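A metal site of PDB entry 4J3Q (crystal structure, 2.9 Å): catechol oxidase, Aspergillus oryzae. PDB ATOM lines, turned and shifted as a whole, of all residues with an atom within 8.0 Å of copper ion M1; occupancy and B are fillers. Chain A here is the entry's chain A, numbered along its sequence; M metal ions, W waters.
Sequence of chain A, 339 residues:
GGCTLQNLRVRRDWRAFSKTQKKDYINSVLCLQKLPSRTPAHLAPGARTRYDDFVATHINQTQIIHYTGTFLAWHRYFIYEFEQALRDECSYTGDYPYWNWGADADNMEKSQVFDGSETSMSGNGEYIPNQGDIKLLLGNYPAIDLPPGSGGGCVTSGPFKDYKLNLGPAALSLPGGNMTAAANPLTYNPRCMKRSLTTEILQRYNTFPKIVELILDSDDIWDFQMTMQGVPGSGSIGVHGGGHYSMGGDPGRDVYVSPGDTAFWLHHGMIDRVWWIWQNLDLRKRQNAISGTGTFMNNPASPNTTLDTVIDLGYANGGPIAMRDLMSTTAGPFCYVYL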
ATOM      1  N   HIS A  58     -19.445   3.505   2.447  1.00  0.00           N
ATOM      2  CA  HIS A  58     -19.267   4.373   1.274  1.00  0.00           C
ATOM      3  C   HIS A  58     -20.366   4.125   0.234  1.00  0.00           C
ATOM      4  O   HIS A  58     -20.977   5.070  -0.270  1.00  0.00           O
ATOM      5  CB  HIS A  58     -17.894   4.165   0.650  1.00  0.00           C
ATOM      6  CG  HIS A  58     -17.487   5.236  -0.318  1.00  0.00           C
ATOM      7  ND1 HIS A  58     -17.723   5.141  -1.677  1.00  0.00           N
ATOM      8  CD2 HIS A  58     -16.836   6.401  -0.131  1.00  0.00           C
ATOM      9  CE1 HIS A  58     -17.258   6.223  -2.273  1.00  0.00           C
ATOM     10  NE2 HIS A  58     -16.708   6.996  -1.352  1.00  0.00           N
ATOM     11  N   ILE A  59     -20.591   2.840  -0.076  1.00  0.00           N
ATOM     12  CA  ILE A  59     -21.738   2.400  -0.878  1.00  0.00           C
ATOM     13  C   ILE A  59     -23.026   2.926  -0.254  1.00  0.00           C
ATOM     14  O   ILE A  59     -23.840   3.532  -0.927  1.00  0.00           O
ATOM     15  CB  ILE A  59     -21.802   0.861  -0.976  1.00  0.00           C
ATOM     16  CG1 ILE A  59     -20.622   0.307  -1.810  1.00  0.00           C
ATOM     17  CG2 ILE A  59     -23.178   0.389  -1.540  1.00  0.00           C
ATOM     18  CD1 ILE A  59     -20.277  -1.163  -1.519  1.00  0.00           C
ATOM     19  N   GLN A  61     -23.594   5.411   1.598  1.00  0.00           N
ATOM     20  CA  GLN A  61     -23.770   6.866   1.718  1.00  0.00           C
ATOM     21  C   GLN A  61     -23.432   7.648   0.464  1.00  0.00           C
ATOM     22  O   GLN A  61     -23.483   8.866   0.484  1.00  0.00           O
ATOM     23  CB  GLN A  61     -22.948   7.406   2.892  1.00  0.00           C
ATOM     24  CG  GLN A  61     -23.389   6.907   4.250  1.00  0.00           C
ATOM     25  CD  GLN A  61     -22.688   7.622   5.380  1.00  0.00           C
ATOM     26  OE1 GLN A  61     -22.664   8.853   5.426  1.00  0.00           O
ATOM     27  NE2 GLN A  61     -22.128   6.868   6.301  1.00  0.00           N
ATOM     28  N   THR A  62     -23.087   6.974  -0.625  1.00  0.00           N
ATOM     29  CA  THR A  62     -22.555   7.649  -1.808  1.00  0.00           C
ATOM     30  C   THR A  62     -23.422   8.801  -2.325  1.00  0.00           C
ATOM     31  O   THR A  62     -22.886   9.834  -2.712  1.00  0.00           O
ATOM     32  CB  THR A  62     -22.232   6.626  -2.922  1.00  0.00           C
ATOM     33  OG1 THR A  62     -21.010   5.971  -2.584  1.00  0.00           O
ATOM     34  CG2 THR A  62     -22.069   7.286  -4.273  1.00  0.00           C
ATOM     35  N   ILE A  65     -22.766  12.193  -0.179  1.00  0.00           N
ATOM     36  CA  ILE A  65     -21.369  12.520   0.151  1.00  0.00           C
ATOM     37  C   ILE A  65     -20.515  12.885  -1.061  1.00  0.00           C
ATOM     38  O   ILE A  65     -19.318  13.066  -0.931  1.00  0.00           O
ATOM     39  CB  ILE A  65     -20.631  11.382   0.907  1.00  0.00           C
ATOM     40  CG1 ILE A  65     -20.436  10.204  -0.006  1.00  0.00           C
ATOM     41  CG2 ILE A  65     -21.371  10.948   2.078  1.00  0.00           C
ATOM     42  CD1 ILE A  65     -19.580   9.077   0.568  1.00  0.00           C
ATOM     43  N   HIS A  66     -21.113  12.994  -2.234  1.00  0.00           N
ATOM     44  CA  HIS A  66     -20.401  13.467  -3.389  1.00  0.00           C
ATOM     45  C   HIS A  66     -21.300  14.539  -3.988  1.00  0.00           C
ATOM     46  O   HIS A  66     -22.501  14.324  -4.069  1.00  0.00           O
ATOM     47  CB  HIS A  66     -20.120  12.314  -4.373  1.00  0.00           C
ATOM     48  CG  HIS A  66     -19.247  11.227  -3.807  1.00  0.00           C
ATOM     49  ND1 HIS A  66     -19.747  10.015  -3.409  1.00  0.00           N
ATOM     50  CD2 HIS A  66     -17.906  11.170  -3.580  1.00  0.00           C
ATOM     51  CE1 HIS A  66     -18.756   9.250  -2.961  1.00  0.00           C
ATOM     52  NE2 HIS A  66     -17.619   9.938  -3.043  1.00  0.00           N
ATOM     53  N   PHE A  71     -18.991  16.827   1.276  1.00  0.00           N
ATOM     54  CA  PHE A  71     -18.037  15.998   0.527  1.00  0.00           C
ATOM     55  C   PHE A  71     -16.649  16.032   1.111  1.00  0.00           C
ATOM     56  O   PHE A  71     -16.115  14.997   1.486  1.00  0.00           O
ATOM     57  CB  PHE A  71     -18.013  16.410  -0.958  1.00  0.00           C
ATOM     58  CG  PHE A  71     -16.819  15.942  -1.746  1.00  0.00           C
ATOM     59  CD1 PHE A  71     -16.636  14.609  -2.035  1.00  0.00           C
ATOM     60  CD2 PHE A  71     -15.917  16.872  -2.261  1.00  0.00           C
ATOM     61  CE1 PHE A  71     -15.555  14.182  -2.795  1.00  0.00           C
ATOM     62  CE2 PHE A  71     -14.818  16.450  -3.036  1.00  0.00           C
ATOM     63  CZ  PHE A  71     -14.644  15.097  -3.298  1.00  0.00           C
ATOM     64  N   TRP A  74     -16.658  15.036   4.939  1.00  0.00           N
ATOM     65  CA  TRP A  74     -17.017  13.656   5.194  1.00  0.00           C
ATOM     66  C   TRP A  74     -15.852  12.791   4.826  1.00  0.00           C
ATOM     67  O   TRP A  74     -15.467  11.952   5.610  1.00  0.00           O
ATOM     68  CB  TRP A  74     -18.281  13.261   4.452  1.00  0.00           C
ATOM     69  CG  TRP A  74     -18.738  11.867   4.706  1.00  0.00           C
ATOM     70  CD1 TRP A  74     -19.758  11.476   5.540  1.00  0.00           C
ATOM     71  CD2 TRP A  74     -18.216  10.680   4.108  1.00  0.00           C
ATOM     72  NE1 TRP A  74     -19.899  10.112   5.495  1.00  0.00           N
ATOM     73  CE2 TRP A  74     -18.957   9.599   4.619  1.00  0.00           C
ATOM     74  CE3 TRP A  74     -17.200  10.415   3.169  1.00  0.00           C
ATOM     75  CZ2 TRP A  74     -18.706   8.269   4.232  1.00  0.00           C
ATOM     76  CZ3 TRP A  74     -16.944   9.099   2.791  1.00  0.00           C
ATOM     77  CH2 TRP A  74     -17.691   8.040   3.327  1.00  0.00           C
ATOM     78  N   HIS A  75     -15.224  13.043   3.693  1.00  0.00           N
ATOM     79  CA  HIS A  75     -14.031  12.281   3.335  1.00  0.00           C
ATOM     80  C   HIS A  75     -12.844  12.472   4.265  1.00  0.00           C
ATOM     81  O   HIS A  75     -12.038  11.552   4.465  1.00  0.00           O
ATOM     82  CB  HIS A  75     -13.642  12.562   1.881  1.00  0.00           C
ATOM     83  CG  HIS A  75     -14.518  11.819   0.920  1.00  0.00           C
ATOM     84  ND1 HIS A  75     -15.672  12.353   0.402  1.00  0.00           N
ATOM     85  CD2 HIS A  75     -14.465  10.535   0.499  1.00  0.00           C
ATOM     86  CE1 HIS A  75     -16.265  11.440  -0.362  1.00  0.00           C
ATOM     87  NE2 HIS A  75     -15.555  10.338  -0.300  1.00  0.00           N
ATOM     88  N   PHE A  78     -13.657  10.222   7.107  1.00  0.00           N
ATOM     89  CA  PHE A  78     -13.597   8.871   6.657  1.00  0.00           C
ATOM     90  C   PHE A  78     -12.170   8.376   6.750  1.00  0.00           C
ATOM     91  O   PHE A  78     -11.908   7.444   7.502  1.00  0.00           O
ATOM     92  CB  PHE A  78     -14.067   8.851   5.230  1.00  0.00           C
ATOM     93  CG  PHE A  78     -14.359   7.496   4.715  1.00  0.00           C
ATOM     94  CD1 PHE A  78     -15.135   6.607   5.419  1.00  0.00           C
ATOM     95  CD2 PHE A  78     -13.887   7.129   3.446  1.00  0.00           C
ATOM     96  CE1 PHE A  78     -15.426   5.341   4.905  1.00  0.00           C
ATOM     97  CE2 PHE A  78     -14.178   5.881   2.924  1.00  0.00           C
ATOM     98  CZ  PHE A  78     -14.954   4.983   3.657  1.00  0.00           C
ATOM     99  N   GLN A 229     -14.219  18.196  -8.205  1.00  0.00           N
ATOM    100  CA  GLN A 229     -15.047  17.008  -8.484  1.00  0.00           C
ATOM    101  C   GLN A 229     -15.389  16.898  -9.922  1.00  0.00           C
ATOM    102  O   GLN A 229     -15.621  15.792 -10.422  1.00  0.00           O
ATOM    103  CB  GLN A 229     -16.327  17.034  -7.682  1.00  0.00           C
ATOM    104  CG  GLN A 229     -16.076  16.733  -6.257  1.00  0.00           C
ATOM    105  CD  GLN A 229     -17.317  16.736  -5.434  1.00  0.00           C
ATOM    106  OE1 GLN A 229     -17.979  15.681  -5.269  1.00  0.00           O
ATOM    107  NE2 GLN A 229     -17.645  17.891  -4.895  1.00  0.00           N
ATOM    108  N   HIS A 240     -10.149  14.963  -8.547  1.00  0.00           N
ATOM    109  CA  HIS A 240     -10.785  13.859  -7.843  1.00  0.00           C
ATOM    110  C   HIS A 240     -11.262  12.735  -8.771  1.00  0.00           C
ATOM    111  O   HIS A 240     -11.135  11.559  -8.447  1.00  0.00           O
ATOM    112  CB  HIS A 240     -11.936  14.365  -6.973  1.00  0.00           C
ATOM    113  CG  HIS A 240     -12.719  13.268  -6.320  1.00  0.00           C
ATOM    114  ND1 HIS A 240     -13.965  12.880  -6.771  1.00  0.00           N
ATOM    115  CD2 HIS A 240     -12.408  12.428  -5.309  1.00  0.00           C
ATOM    116  CE1 HIS A 240     -14.398  11.869  -6.040  1.00  0.00           C
ATOM    117  NE2 HIS A 240     -13.465  11.570  -5.146  1.00  0.00           N
ATOM    118  N   HIS A 244      -9.440   8.818  -9.620  1.00  0.00           N
ATOM    119  CA  HIS A 244     -10.180   7.566  -9.552  1.00  0.00           C
ATOM    120  C   HIS A 244     -10.108   6.803 -10.857  1.00  0.00           C
ATOM    121  O   HIS A 244      -9.718   5.636 -10.877  1.00  0.00           O
ATOM    122  CB  HIS A 244     -11.632   7.784  -9.100  1.00  0.00           C
ATOM    123  CG  HIS A 244     -11.779   7.913  -7.619  1.00  0.00           C
ATOM    124  ND1 HIS A 244     -11.262   6.989  -6.736  1.00  0.00           N
ATOM    125  CD2 HIS A 244     -12.368   8.872  -6.864  1.00  0.00           C
ATOM    126  CE1 HIS A 244     -11.529   7.367  -5.502  1.00  0.00           C
ATOM    127  NE2 HIS A 244     -12.208   8.500  -5.547  1.00  0.00           N
ATOM    128  N   ASP A 254     -16.062   2.569 -10.231  1.00  0.00           N
ATOM    129  CA  ASP A 254     -17.328   2.576  -9.498  1.00  0.00           C
ATOM    130  C   ASP A 254     -17.317   3.690  -8.441  1.00  0.00           C
ATOM    131  O   ASP A 254     -16.584   3.624  -7.453  1.00  0.00           O
ATOM    132  CB  ASP A 254     -17.549   1.197  -8.845  1.00  0.00           C
ATOM    133  CG  ASP A 254     -19.016   0.894  -8.538  1.00  0.00           C
ATOM    134  OD1 ASP A 254     -19.771   1.817  -8.133  1.00  0.00           O
ATOM    135  OD2 ASP A 254     -19.416  -0.287  -8.674  1.00  0.00           O
ATOM    136  N   VAL A 255     -18.117   4.722  -8.635  1.00  0.00           N
ATOM    137  CA  VAL A 255     -18.252   5.799  -7.658  1.00  0.00           C
ATOM    138  C   VAL A 255     -18.596   5.313  -6.226  1.00  0.00           C
ATOM    139  O   VAL A 255     -18.173   5.951  -5.259  1.00  0.00           O
ATOM    140  CB  VAL A 255     -19.323   6.839  -8.096  1.00  0.00           C
ATOM    141  CG1 VAL A 255     -19.468   7.931  -7.057  1.00  0.00           C
ATOM    142  CG2 VAL A 255     -18.983   7.443  -9.458  1.00  0.00           C
ATOM    143  N   TYR A 256     -19.351   4.232  -6.090  1.00  0.00           N
ATOM    144  CA  TYR A 256     -19.778   3.759  -4.773  1.00  0.00           C
ATOM    145  C   TYR A 256     -18.751   2.863  -4.077  1.00  0.00           C
ATOM    146  O   TYR A 256     -18.544   2.976  -2.877  1.00  0.00           O
ATOM    147  CB  TYR A 256     -21.038   2.920  -4.858  1.00  0.00           C
ATOM    148  CG  TYR A 256     -22.289   3.565  -5.392  1.00  0.00           C
ATOM    149  CD1 TYR A 256     -23.411   3.683  -4.587  1.00  0.00           C
ATOM    150  CD2 TYR A 256     -22.387   3.961  -6.732  1.00  0.00           C
ATOM    151  CE1 TYR A 256     -24.584   4.222  -5.068  1.00  0.00           C
ATOM    152  CE2 TYR A 256     -23.574   4.520  -7.218  1.00  0.00           C
ATOM    153  CZ  TYR A 256     -24.656   4.633  -6.376  1.00  0.00           C
ATOM    154  OH  TYR A 256     -25.824   5.177  -6.820  1.00  0.00           O
ATOM    155  N   VAL A 257     -18.149   1.958  -4.835  1.00  0.00           N
ATOM    156  CA  VAL A 257     -17.290   0.928  -4.288  1.00  0.00           C
ATOM    157  C   VAL A 257     -15.807   1.337  -4.275  1.00  0.00           C
ATOM    158  O   VAL A 257     -14.960   0.585  -3.792  1.00  0.00           O
ATOM    159  CB  VAL A 257     -17.500  -0.415  -5.056  1.00  0.00           C
ATOM    160  CG1 VAL A 257     -16.984  -1.605  -4.258  1.00  0.00           C
ATOM    161  CG2 VAL A 257     -18.958  -0.624  -5.361  1.00  0.00           C
ATOM    162  N   SER A 258     -15.500   2.556  -4.749  1.00  0.00           N
ATOM    163  CA  SER A 258     -14.115   3.036  -4.920  1.00  0.00           C
ATOM    164  C   SER A 258     -13.106   2.771  -3.776  1.00  0.00           C
ATOM    165  O   SER A 258     -11.936   2.481  -4.052  1.00  0.00           O
ATOM    166  CB  SER A 258     -14.064   4.489  -5.370  1.00  0.00           C
ATOM    167  OG  SER A 258     -14.787   5.324  -4.491  1.00  0.00           O
ATOM    168  N   PRO A 259     -13.543   2.843  -2.511  1.00  0.00           N
ATOM    169  CA  PRO A 259     -12.680   2.379  -1.415  1.00  0.00           C
ATOM    170  C   PRO A 259     -12.213   0.923  -1.552  1.00  0.00           C
ATOM    171  O   PRO A 259     -11.319   0.487  -0.844  1.00  0.00           O
ATOM    172  CB  PRO A 259     -13.566   2.521  -0.191  1.00  0.00           C
ATOM    173  CG  PRO A 259     -14.433   3.626  -0.516  1.00  0.00           C
ATOM    174  CD  PRO A 259     -14.736   3.521  -1.970  1.00  0.00           C
ATOM    175  N   PHE A 264      -7.360   4.153  -2.851  1.00  0.00           N
ATOM    176  CA  PHE A 264      -8.354   5.144  -2.452  1.00  0.00           C
ATOM    177  C   PHE A 264      -7.829   6.094  -1.374  1.00  0.00           C
ATOM    178  O   PHE A 264      -7.883   7.299  -1.534  1.00  0.00           O
ATOM    179  CB  PHE A 264      -9.590   4.462  -1.926  1.00  0.00           C
ATOM    180  CG  PHE A 264     -10.642   5.407  -1.405  1.00  0.00           C
ATOM    181  CD1 PHE A 264     -10.707   5.726  -0.068  1.00  0.00           C
ATOM    182  CD2 PHE A 264     -11.599   5.930  -2.260  1.00  0.00           C
ATOM    183  CE1 PHE A 264     -11.697   6.552   0.403  1.00  0.00           C
ATOM    184  CE2 PHE A 264     -12.585   6.753  -1.797  1.00  0.00           C
ATOM    185  CZ  PHE A 264     -12.645   7.059  -0.464  1.00  0.00           C
ATOM    186  N   HIS A 268      -7.200   9.988  -1.506  1.00  0.00           N
ATOM    187  CA  HIS A 268      -7.948  10.970  -0.716  1.00  0.00           C
ATOM    188  C   HIS A 268      -7.090  11.708   0.310  1.00  0.00           C
ATOM    189  O   HIS A 268      -7.509  12.736   0.838  1.00  0.00           O
ATOM    190  CB  HIS A 268      -9.169  10.345  -0.034  1.00  0.00           C
ATOM    191  CG  HIS A 268     -10.410  10.407  -0.856  1.00  0.00           C
ATOM    192  ND1 HIS A 268     -11.236  11.509  -0.863  1.00  0.00           N
ATOM    193  CD2 HIS A 268     -10.961   9.518  -1.717  1.00  0.00           C
ATOM    194  CE1 HIS A 268     -12.236  11.296  -1.701  1.00  0.00           C
ATOM    195  NE2 HIS A 268     -12.098  10.083  -2.214  1.00  0.00           N
HETATM  196 CU    CU M   1     -16.308   9.007  -1.641  1.00  0.00          CU
HETATM  197 CU    CU M   2     -12.849   9.868  -4.124  1.00  0.00          CU
HETATM  198  O   HOH W   1     -15.041   8.900  -3.755  1.00  0.00           O
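Residues that only touch copper ion M1: Ile 65 (3.9 Å). Four residues have an atom within 4 Å of copper ion M1: His 58, Ile 65, His 66 and His 75. The nearest printed residue that does not touch copper ion M1 is Phe 264 (4.3 Å).
A ring nitrogen (ND1) of His 58 is in hydrogen-bond range of the backbone carbonyl oxygen of Tyr 256, at 2.6 Å. O of His 58 sits at hydrogen-bond distance from OG1 of Thr 62 (2.5 Å). O of Thr 62 is in hydrogen-bond range of ND1 of His 66, 3.2 Å away. A ring nitrogen (ND1) of His 75 sits at hydrogen-bond distance from the backbone carbonyl oxygen (O) of Phe 71, 2.9 Å away.
Copper ion M1 is bound by NE2 of His 75 (2.0 Å), NE2 of His 58 (2.1 Å), NE2 of His 66 (2.1 Å) and water W1 (2.5 Å).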
